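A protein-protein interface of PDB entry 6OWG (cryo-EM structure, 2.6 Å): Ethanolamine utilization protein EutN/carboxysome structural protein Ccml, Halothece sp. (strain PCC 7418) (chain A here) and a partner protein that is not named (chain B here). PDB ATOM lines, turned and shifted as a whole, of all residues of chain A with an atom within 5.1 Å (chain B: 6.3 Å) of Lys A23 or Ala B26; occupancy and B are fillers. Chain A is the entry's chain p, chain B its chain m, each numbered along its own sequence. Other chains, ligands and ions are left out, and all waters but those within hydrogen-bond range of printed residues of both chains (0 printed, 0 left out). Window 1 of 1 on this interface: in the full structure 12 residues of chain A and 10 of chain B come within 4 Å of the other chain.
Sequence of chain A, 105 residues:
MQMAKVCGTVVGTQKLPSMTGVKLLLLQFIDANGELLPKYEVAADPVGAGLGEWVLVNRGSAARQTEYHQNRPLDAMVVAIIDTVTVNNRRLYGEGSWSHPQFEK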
ATOM      1  N   THR A   9      -9.274  23.960   1.668  1.00  0.00           N
ATOM      2  CA  THR A   9      -9.429  23.110   0.499  1.00  0.00           C
ATOM      3  C   THR A   9      -8.066  22.622   0.040  1.00  0.00           C
ATOM      4  O   THR A   9      -7.064  23.325   0.184  1.00  0.00           O
ATOM      5  CB  THR A   9     -10.120  23.849  -0.663  1.00  0.00           C
ATOM      6  OG1 THR A   9      -9.339  24.987  -1.047  1.00  0.00           O
ATOM      7  CG2 THR A   9     -11.505  24.313  -0.269  1.00  0.00           C
ATOM      8  N   VAL A  11      -6.342  21.181  -3.456  1.00  0.00           N
ATOM      9  CA  VAL A  11      -6.490  21.016  -4.894  1.00  0.00           C
ATOM     10  C   VAL A  11      -5.274  20.258  -5.402  1.00  0.00           C
ATOM     11  O   VAL A  11      -4.135  20.676  -5.170  1.00  0.00           O
ATOM     12  CB  VAL A  11      -6.642  22.366  -5.614  1.00  0.00           C
ATOM     13  CG1 VAL A  11      -6.450  22.208  -7.110  1.00  0.00           C
ATOM     14  CG2 VAL A  11      -8.004  22.969  -5.317  1.00  0.00           C
ATOM     15  N   GLY A  21     -13.313  15.084 -10.169  1.00  0.00           N
ATOM     16  CA  GLY A  21     -14.631  15.459  -9.709  1.00  0.00           C
ATOM     17  C   GLY A  21     -14.827  15.409  -8.211  1.00  0.00           C
ATOM     18  O   GLY A  21     -15.879  15.844  -7.728  1.00  0.00           O
ATOM     19  N   VAL A  22     -13.852  14.905  -7.461  1.00  0.00           N
ATOM     20  CA  VAL A  22     -13.948  14.756  -6.016  1.00  0.00           C
ATOM     21  C   VAL A  22     -13.465  16.045  -5.373  1.00  0.00           C
ATOM     22  O   VAL A  22     -12.309  16.447  -5.555  1.00  0.00           O
ATOM     23  CB  VAL A  22     -13.130  13.551  -5.526  1.00  0.00           C
ATOM     24  CG1 VAL A  22     -13.098  13.509  -4.014  1.00  0.00           C
ATOM     25  CG2 VAL A  22     -13.700  12.260  -6.082  1.00  0.00           C
ATOM     26  N   LYS A  23     -14.349  16.699  -4.627  1.00  0.00           N
ATOM     27  CA  LYS A  23     -13.998  17.911  -3.902  1.00  0.00           C
ATOM     28  C   LYS A  23     -13.327  17.525  -2.590  1.00  0.00           C
ATOM     29  O   LYS A  23     -13.877  16.739  -1.816  1.00  0.00           O
ATOM     30  CB  LYS A  23     -15.245  18.754  -3.660  1.00  0.00           C
ATOM     31  CG  LYS A  23     -15.076  19.870  -2.656  1.00  0.00           C
ATOM     32  CD  LYS A  23     -16.427  20.433  -2.264  1.00  0.00           C
ATOM     33  CE  LYS A  23     -16.298  21.473  -1.171  1.00  0.00           C
ATOM     34  NZ  LYS A  23     -17.613  21.798  -0.560  1.00  0.00           N
ATOM     35  N   LEU A  24     -12.142  18.072  -2.345  1.00  0.00           N
ATOM     36  CA  LEU A  24     -11.310  17.681  -1.217  1.00  0.00           C
ATOM     37  C   LEU A  24     -11.212  18.826  -0.223  1.00  0.00           C
ATOM     38  O   LEU A  24     -10.702  19.899  -0.556  1.00  0.00           O
ATOM     39  CB  LEU A  24      -9.916  17.276  -1.690  1.00  0.00           C
ATOM     40  CG  LEU A  24      -9.899  16.134  -2.700  1.00  0.00           C
ATOM     41  CD1 LEU A  24      -8.586  16.115  -3.442  1.00  0.00           C
ATOM     42  CD2 LEU A  24     -10.145  14.817  -2.000  1.00  0.00           C
ATOM     43  N   LEU A  25     -11.694  18.594   0.988  1.00  0.00           N
ATOM     44  CA  LEU A  25     -11.679  19.589   2.044  1.00  0.00           C
ATOM     45  C   LEU A  25     -10.637  19.231   3.090  1.00  0.00           C
ATOM     46  O   LEU A  25     -10.506  18.082   3.506  1.00  0.00           O
ATOM     47  CB  LEU A  25     -13.058  19.705   2.698  1.00  0.00           C
ATOM     48  CG  LEU A  25     -14.151  20.415   1.910  1.00  0.00           C
ATOM     49  CD1 LEU A  25     -15.373  20.554   2.773  1.00  0.00           C
ATOM     50  CD2 LEU A  25     -13.669  21.770   1.455  1.00  0.00           C
ATOM     51  N   ALA A  43     -10.865  15.024   3.190  1.00  0.00           N
ATOM     52  CA  ALA A  43     -12.037  14.202   2.955  1.00  0.00           C
ATOM     53  C   ALA A  43     -12.750  14.633   1.686  1.00  0.00           C
ATOM     54  O   ALA A  43     -12.709  15.799   1.293  1.00  0.00           O
ATOM     55  CB  ALA A  43     -13.007  14.271   4.128  1.00  0.00           C
ATOM     56  N   ALA A  44     -13.398  13.665   1.046  1.00  0.00           N
ATOM     57  CA  ALA A  44     -14.342  13.960  -0.015  1.00  0.00           C
ATOM     58  C   ALA A  44     -15.575  14.638   0.565  1.00  0.00           C
ATOM     59  O   ALA A  44     -15.993  14.357   1.689  1.00  0.00           O
ATOM     60  CB  ALA A  44     -14.741  12.682  -0.745  1.00  0.00           C
ATOM     61  N   ASP A  45     -16.166  15.542  -0.213  1.00  0.00           N
ATOM     62  CA  ASP A  45     -17.263  16.381   0.257  1.00  0.00           C
ATOM     63  C   ASP A  45     -18.457  16.267  -0.686  1.00  0.00           C
ATOM     64  O   ASP A  45     -18.619  17.090  -1.599  1.00  0.00           O
ATOM     65  CB  ASP A  45     -16.804  17.829   0.390  1.00  0.00           C
ATOM     66  CG  ASP A  45     -17.843  18.706   1.029  1.00  0.00           C
ATOM     67  OD1 ASP A  45     -18.007  18.623   2.259  1.00  0.00           O
ATOM     68  OD2 ASP A  45     -18.494  19.484   0.305  1.00  0.00           O
ATOM     69  N   VAL A  47     -21.704  16.344   0.543  1.00  0.00           N
ATOM     70  CA  VAL A  47     -22.592  17.321   1.159  1.00  0.00           C
ATOM     71  C   VAL A  47     -21.840  18.640   1.181  1.00  0.00           C
ATOM     72  O   VAL A  47     -20.830  18.757   1.880  1.00  0.00           O
ATOM     73  CB  VAL A  47     -22.994  16.893   2.579  1.00  0.00           C
ATOM     74  CG1 VAL A  47     -24.090  17.787   3.114  1.00  0.00           C
ATOM     75  CG2 VAL A  47     -23.411  15.433   2.600  1.00  0.00           C
ATOM     76  N   GLY A  48     -22.336  19.625   0.433  1.00  0.00           N
ATOM     77  CA  GLY A  48     -21.548  20.810   0.122  1.00  0.00           C
ATOM     78  C   GLY A  48     -21.264  21.664   1.342  1.00  0.00           C
ATOM     79  O   GLY A  48     -22.163  22.352   1.852  1.00  0.00           O
ATOM     80  N   ALA A  49     -20.019  21.648   1.808  1.00  0.00           N
ATOM     81  CA  ALA A  49     -19.627  22.276   3.059  1.00  0.00           C
ATOM     82  C   ALA A  49     -18.571  23.334   2.790  1.00  0.00           C
ATOM     83  O   ALA A  49     -17.609  23.086   2.057  1.00  0.00           O
ATOM     84  CB  ALA A  49     -19.094  21.241   4.051  1.00  0.00           C
ATOM     85  N   GLY A  50     -18.752  24.510   3.387  1.00  0.00           N
ATOM     86  CA  GLY A  50     -17.833  25.610   3.218  1.00  0.00           C
ATOM     87  C   GLY A  50     -16.978  25.838   4.450  1.00  0.00           C
ATOM     88  O   GLY A  50     -17.107  25.167   5.468  1.00  0.00           O
ATOM     89  N   ASP B  21     -22.289  27.722  -5.777  1.00  0.00           N
ATOM     90  CA  ASP B  21     -21.877  27.506  -4.394  1.00  0.00           C
ATOM     91  C   ASP B  21     -20.781  26.461  -4.286  1.00  0.00           C
ATOM     92  O   ASP B  21     -19.847  26.630  -3.499  1.00  0.00           O
ATOM     93  CB  ASP B  21     -23.071  27.086  -3.541  1.00  0.00           C
ATOM     94  CG  ASP B  21     -22.769  27.105  -2.067  1.00  0.00           C
ATOM     95  OD1 ASP B  21     -22.797  26.020  -1.451  1.00  0.00           O
ATOM     96  OD2 ASP B  21     -22.508  28.198  -1.525  1.00  0.00           O
ATOM     97  N   ALA B  22     -20.874  25.383  -5.064  1.00  0.00           N
ATOM     98  CA  ALA B  22     -19.879  24.323  -4.968  1.00  0.00           C
ATOM     99  C   ALA B  22     -18.574  24.716  -5.641  1.00  0.00           C
ATOM    100  O   ALA B  22     -17.526  24.140  -5.342  1.00  0.00           O
ATOM    101  CB  ALA B  22     -20.417  23.035  -5.577  1.00  0.00           C
ATOM    102  N   MET B  23     -18.615  25.682  -6.560  1.00  0.00           N
ATOM    103  CA  MET B  23     -17.391  26.116  -7.222  1.00  0.00           C
ATOM    104  C   MET B  23     -16.520  26.935  -6.280  1.00  0.00           C
ATOM    105  O   MET B  23     -15.306  26.718  -6.196  1.00  0.00           O
ATOM    106  CB  MET B  23     -17.724  26.912  -8.483  1.00  0.00           C
ATOM    107  CG  MET B  23     -17.928  26.037  -9.700  1.00  0.00           C
ATOM    108  SD  MET B  23     -17.620  26.832 -11.279  1.00  0.00           S
ATOM    109  CE  MET B  23     -19.122  27.769 -11.467  1.00  0.00           C
ATOM    110  N   VAL B  24     -17.121  27.865  -5.540  1.00  0.00           N
ATOM    111  CA  VAL B  24     -16.318  28.705  -4.659  1.00  0.00           C
ATOM    112  C   VAL B  24     -16.036  28.001  -3.342  1.00  0.00           C
ATOM    113  O   VAL B  24     -15.271  28.505  -2.513  1.00  0.00           O
ATOM    114  CB  VAL B  24     -17.007  30.061  -4.441  1.00  0.00           C
ATOM    115  CG1 VAL B  24     -17.064  30.836  -5.740  1.00  0.00           C
ATOM    116  CG2 VAL B  24     -18.384  29.852  -3.897  1.00  0.00           C
ATOM    117  N   LYS B  25     -16.642  26.834  -3.120  1.00  0.00           N
ATOM    118  CA  LYS B  25     -16.338  26.048  -1.933  1.00  0.00           C
ATOM    119  C   LYS B  25     -15.298  24.975  -2.218  1.00  0.00           C
ATOM    120  O   LYS B  25     -14.666  24.463  -1.290  1.00  0.00           O
ATOM    121  CB  LYS B  25     -17.610  25.406  -1.386  1.00  0.00           C
ATOM    122  CG  LYS B  25     -18.410  26.300  -0.480  1.00  0.00           C
ATOM    123  CD  LYS B  25     -19.719  25.648  -0.127  1.00  0.00           C
ATOM    124  CE  LYS B  25     -20.505  26.505   0.832  1.00  0.00           C
ATOM    125  NZ  LYS B  25     -21.905  26.028   0.933  1.00  0.00           N
ATOM    126  N   ALA B  26     -15.113  24.610  -3.488  1.00  0.00           N
ATOM    127  CA  ALA B  26     -14.148  23.567  -3.815  1.00  0.00           C
ATOM    128  C   ALA B  26     -12.738  24.125  -3.917  1.00  0.00           C
ATOM    129  O   ALA B  26     -11.767  23.431  -3.600  1.00  0.00           O
ATOM    130  CB  ALA B  26     -14.529  22.873  -5.119  1.00  0.00           C
ATOM    131  N   ALA B  27     -12.600  25.370  -4.361  1.00  0.00           N
ATOM    132  CA  ALA B  27     -11.292  25.943  -4.620  1.00  0.00           C
ATOM    133  C   ALA B  27     -11.346  27.448  -4.416  1.00  0.00           C
ATOM    134  O   ALA B  27     -12.394  28.020  -4.109  1.00  0.00           O
ATOM    135  CB  ALA B  27     -10.813  25.589  -6.028  1.00  0.00           C
ATOM    136  N   ARG B  28     -10.192  28.088  -4.593  1.00  0.00           N
ATOM    137  CA  ARG B  28     -10.038  29.527  -4.385  1.00  0.00           C
ATOM    138  C   ARG B  28     -10.332  30.239  -5.704  1.00  0.00           C
ATOM    139  O   ARG B  28      -9.450  30.760  -6.389  1.00  0.00           O
ATOM    140  CB  ARG B  28      -8.642  29.830  -3.855  1.00  0.00           C
ATOM    141  CG  ARG B  28      -8.410  31.243  -3.340  1.00  0.00           C
ATOM    142  CD  ARG B  28      -9.528  31.707  -2.434  1.00  0.00           C
ATOM    143  NE  ARG B  28     -10.328  32.737  -3.085  1.00  0.00           N
ATOM    144  CZ  ARG B  28     -11.554  33.080  -2.711  1.00  0.00           C
ATOM    145  NH1 ARG B  28     -12.132  32.468  -1.687  1.00  0.00           N
ATOM    146  NH2 ARG B  28     -12.204  34.029  -3.367  1.00  0.00           N
ATOM    147  N   GLU B  52      -7.284  26.175  -9.616  1.00  0.00           N
ATOM    148  CA  GLU B  52      -8.516  26.386  -8.873  1.00  0.00           C
ATOM    149  C   GLU B  52      -9.742  26.264  -9.766  1.00  0.00           C
ATOM    150  O   GLU B  52     -10.747  25.678  -9.357  1.00  0.00           O
ATOM    151  CB  GLU B  52      -8.484  27.755  -8.200  1.00  0.00           C
ATOM    152  CG  GLU B  52      -7.165  28.078  -7.550  1.00  0.00           C
ATOM    153  CD  GLU B  52      -6.808  27.100  -6.455  1.00  0.00           C
ATOM    154  OE1 GLU B  52      -7.687  26.770  -5.633  1.00  0.00           O
ATOM    155  OE2 GLU B  52      -5.646  26.652  -6.420  1.00  0.00           O
ATOM    156  N   ALA B  55     -10.454  22.689 -10.714  1.00  0.00           N
ATOM    157  CA  ALA B  55     -10.995  21.948  -9.583  1.00  0.00           C
ATOM    158  C   ALA B  55     -12.423  22.373  -9.276  1.00  0.00           C
ATOM    159  O   ALA B  55     -13.252  21.545  -8.887  1.00  0.00           O
ATOM    160  CB  ALA B  55     -10.107  22.141  -8.357  1.00  0.00           C
ATOM    161  N   SER B  56     -12.728  23.659  -9.447  1.00  0.00           N
ATOM    162  CA  SER B  56     -14.054  24.162  -9.112  1.00  0.00           C
ATOM    163  C   SER B  56     -15.096  23.724 -10.133  1.00  0.00           C
ATOM    164  O   SER B  56     -16.194  23.302  -9.757  1.00  0.00           O
ATOM    165  CB  SER B  56     -14.015  25.681  -9.006  1.00  0.00           C
ATOM    166  OG  SER B  56     -14.135  26.279 -10.281  1.00  0.00           O
ATOM    167  N   ALA B  59     -15.794  20.018  -9.805  1.00  0.00           N
ATOM    168  CA  ALA B  59     -16.583  19.718  -8.614  1.00  0.00           C
ATOM    169  C   ALA B  59     -17.952  20.379  -8.681  1.00  0.00           C
ATOM    170  O   ALA B  59     -18.923  19.862  -8.117  1.00  0.00           O
ATOM    171  CB  ALA B  59     -15.837  20.157  -7.359  1.00  0.00           C
ATOM    172  N   GLY B  60     -18.047  21.526  -9.355  1.00  0.00           N
ATOM    173  CA  GLY B  60     -19.337  22.159  -9.549  1.00  0.00           C
ATOM    174  C   GLY B  60     -20.237  21.398 -10.497  1.00  0.00           C
ATOM    175  O   GLY B  60     -21.461  21.501 -10.410  1.00  0.00           O
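The side-chain carboxylate (OD1) of Asp B21 is in salt-bridge range of the side-chain amino group (NZ) of Lys B25 (2.5 Å). N of Arg B28 is in hydrogen-bond range of OE1 of Glu B52 (3.0 Å). N of Leu A25 sits at hydrogen-bond distance from O of Ala A43, 3.0 Å away. The side-chain carboxylate (OD2) of Asp A45 lies within hydrogen-bond range of the backbone NH (N) of Ala A49 (3.0 Å). The side-chain carboxylate (OD2) of Asp A45 is in salt-bridge range of the side-chain amino group (NZ) of Lys A23 (2.6 Å). The backbone carbonyl oxygen of Ala A49 sits at hydrogen-bond distance from the side-chain amino group of Lys A23, 2.9 Å away.
Among the printed residues, merely in contact across the chains: Thr A9 with Lys B25 (3.3 Å), Thr A9 with Ala B26 (3.4 Å), Lys A23 with Lys B25 (3.4 Å), Gly A50 with Lys B25 (3.7 Å), Val A11 with Ala B55 (3.8 Å), Gly A48 with Lys B25 (3.8 Å), Val A11 with Glu B52 (3.8 Å), Ala A49 with Lys B25 (3.9 Å), Val A11 with Ala B27 (3.9 Å), Lys A23 with Ala B26 (3.9 Å) and Leu A25 with Lys B25 (3.97 Å).
Of the printed residues of chain B, Lys A23 touches Lys B25 (3.4 Å) and Ala B26 (3.9 Å). Ala B26 touches just these residues of chain A: Thr A9 and Lys A23. Of the printed residues of chain B, Ala A49 touches Lys B25. Of the printed residues of chain B, Gly A50 touches Lys B25. Of the printed residues of chain B, Val A11 touches Ala B27 (3.9 Å), Glu B52 (3.8 Å) and Ala B55 (3.8 Å). Of the printed residues of chain A, Ala B55 touches Val A11 (3.8 Å). Of the printed residues of chain B, Thr A9 touches Lys B25 and Ala B26. Val A22 touches none of the printed residues of chain B. The nearest residue of chain A that does not touch Ala B26 is Val A11 (4.2 Å).
Of the 14 printed residues of chain A, 7 touch a printed residue of chain B. Printed residues of chain A that touch a printed residue of chain B: Thr A9, Val A11, Lys A23, Leu A25, Gly A48, Ala A49 and Gly A50. Hydrophobic or aromatic side chains of chain A that line the printed part of chain B: Val A11 and Leu A25. Hydrophobic or aromatic side chains of chain B within 4 Å of the printed part of chain A: Ala B26, Ala B27 and Ala B55. Among the printed residues, 11 pairs touch across the chains.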
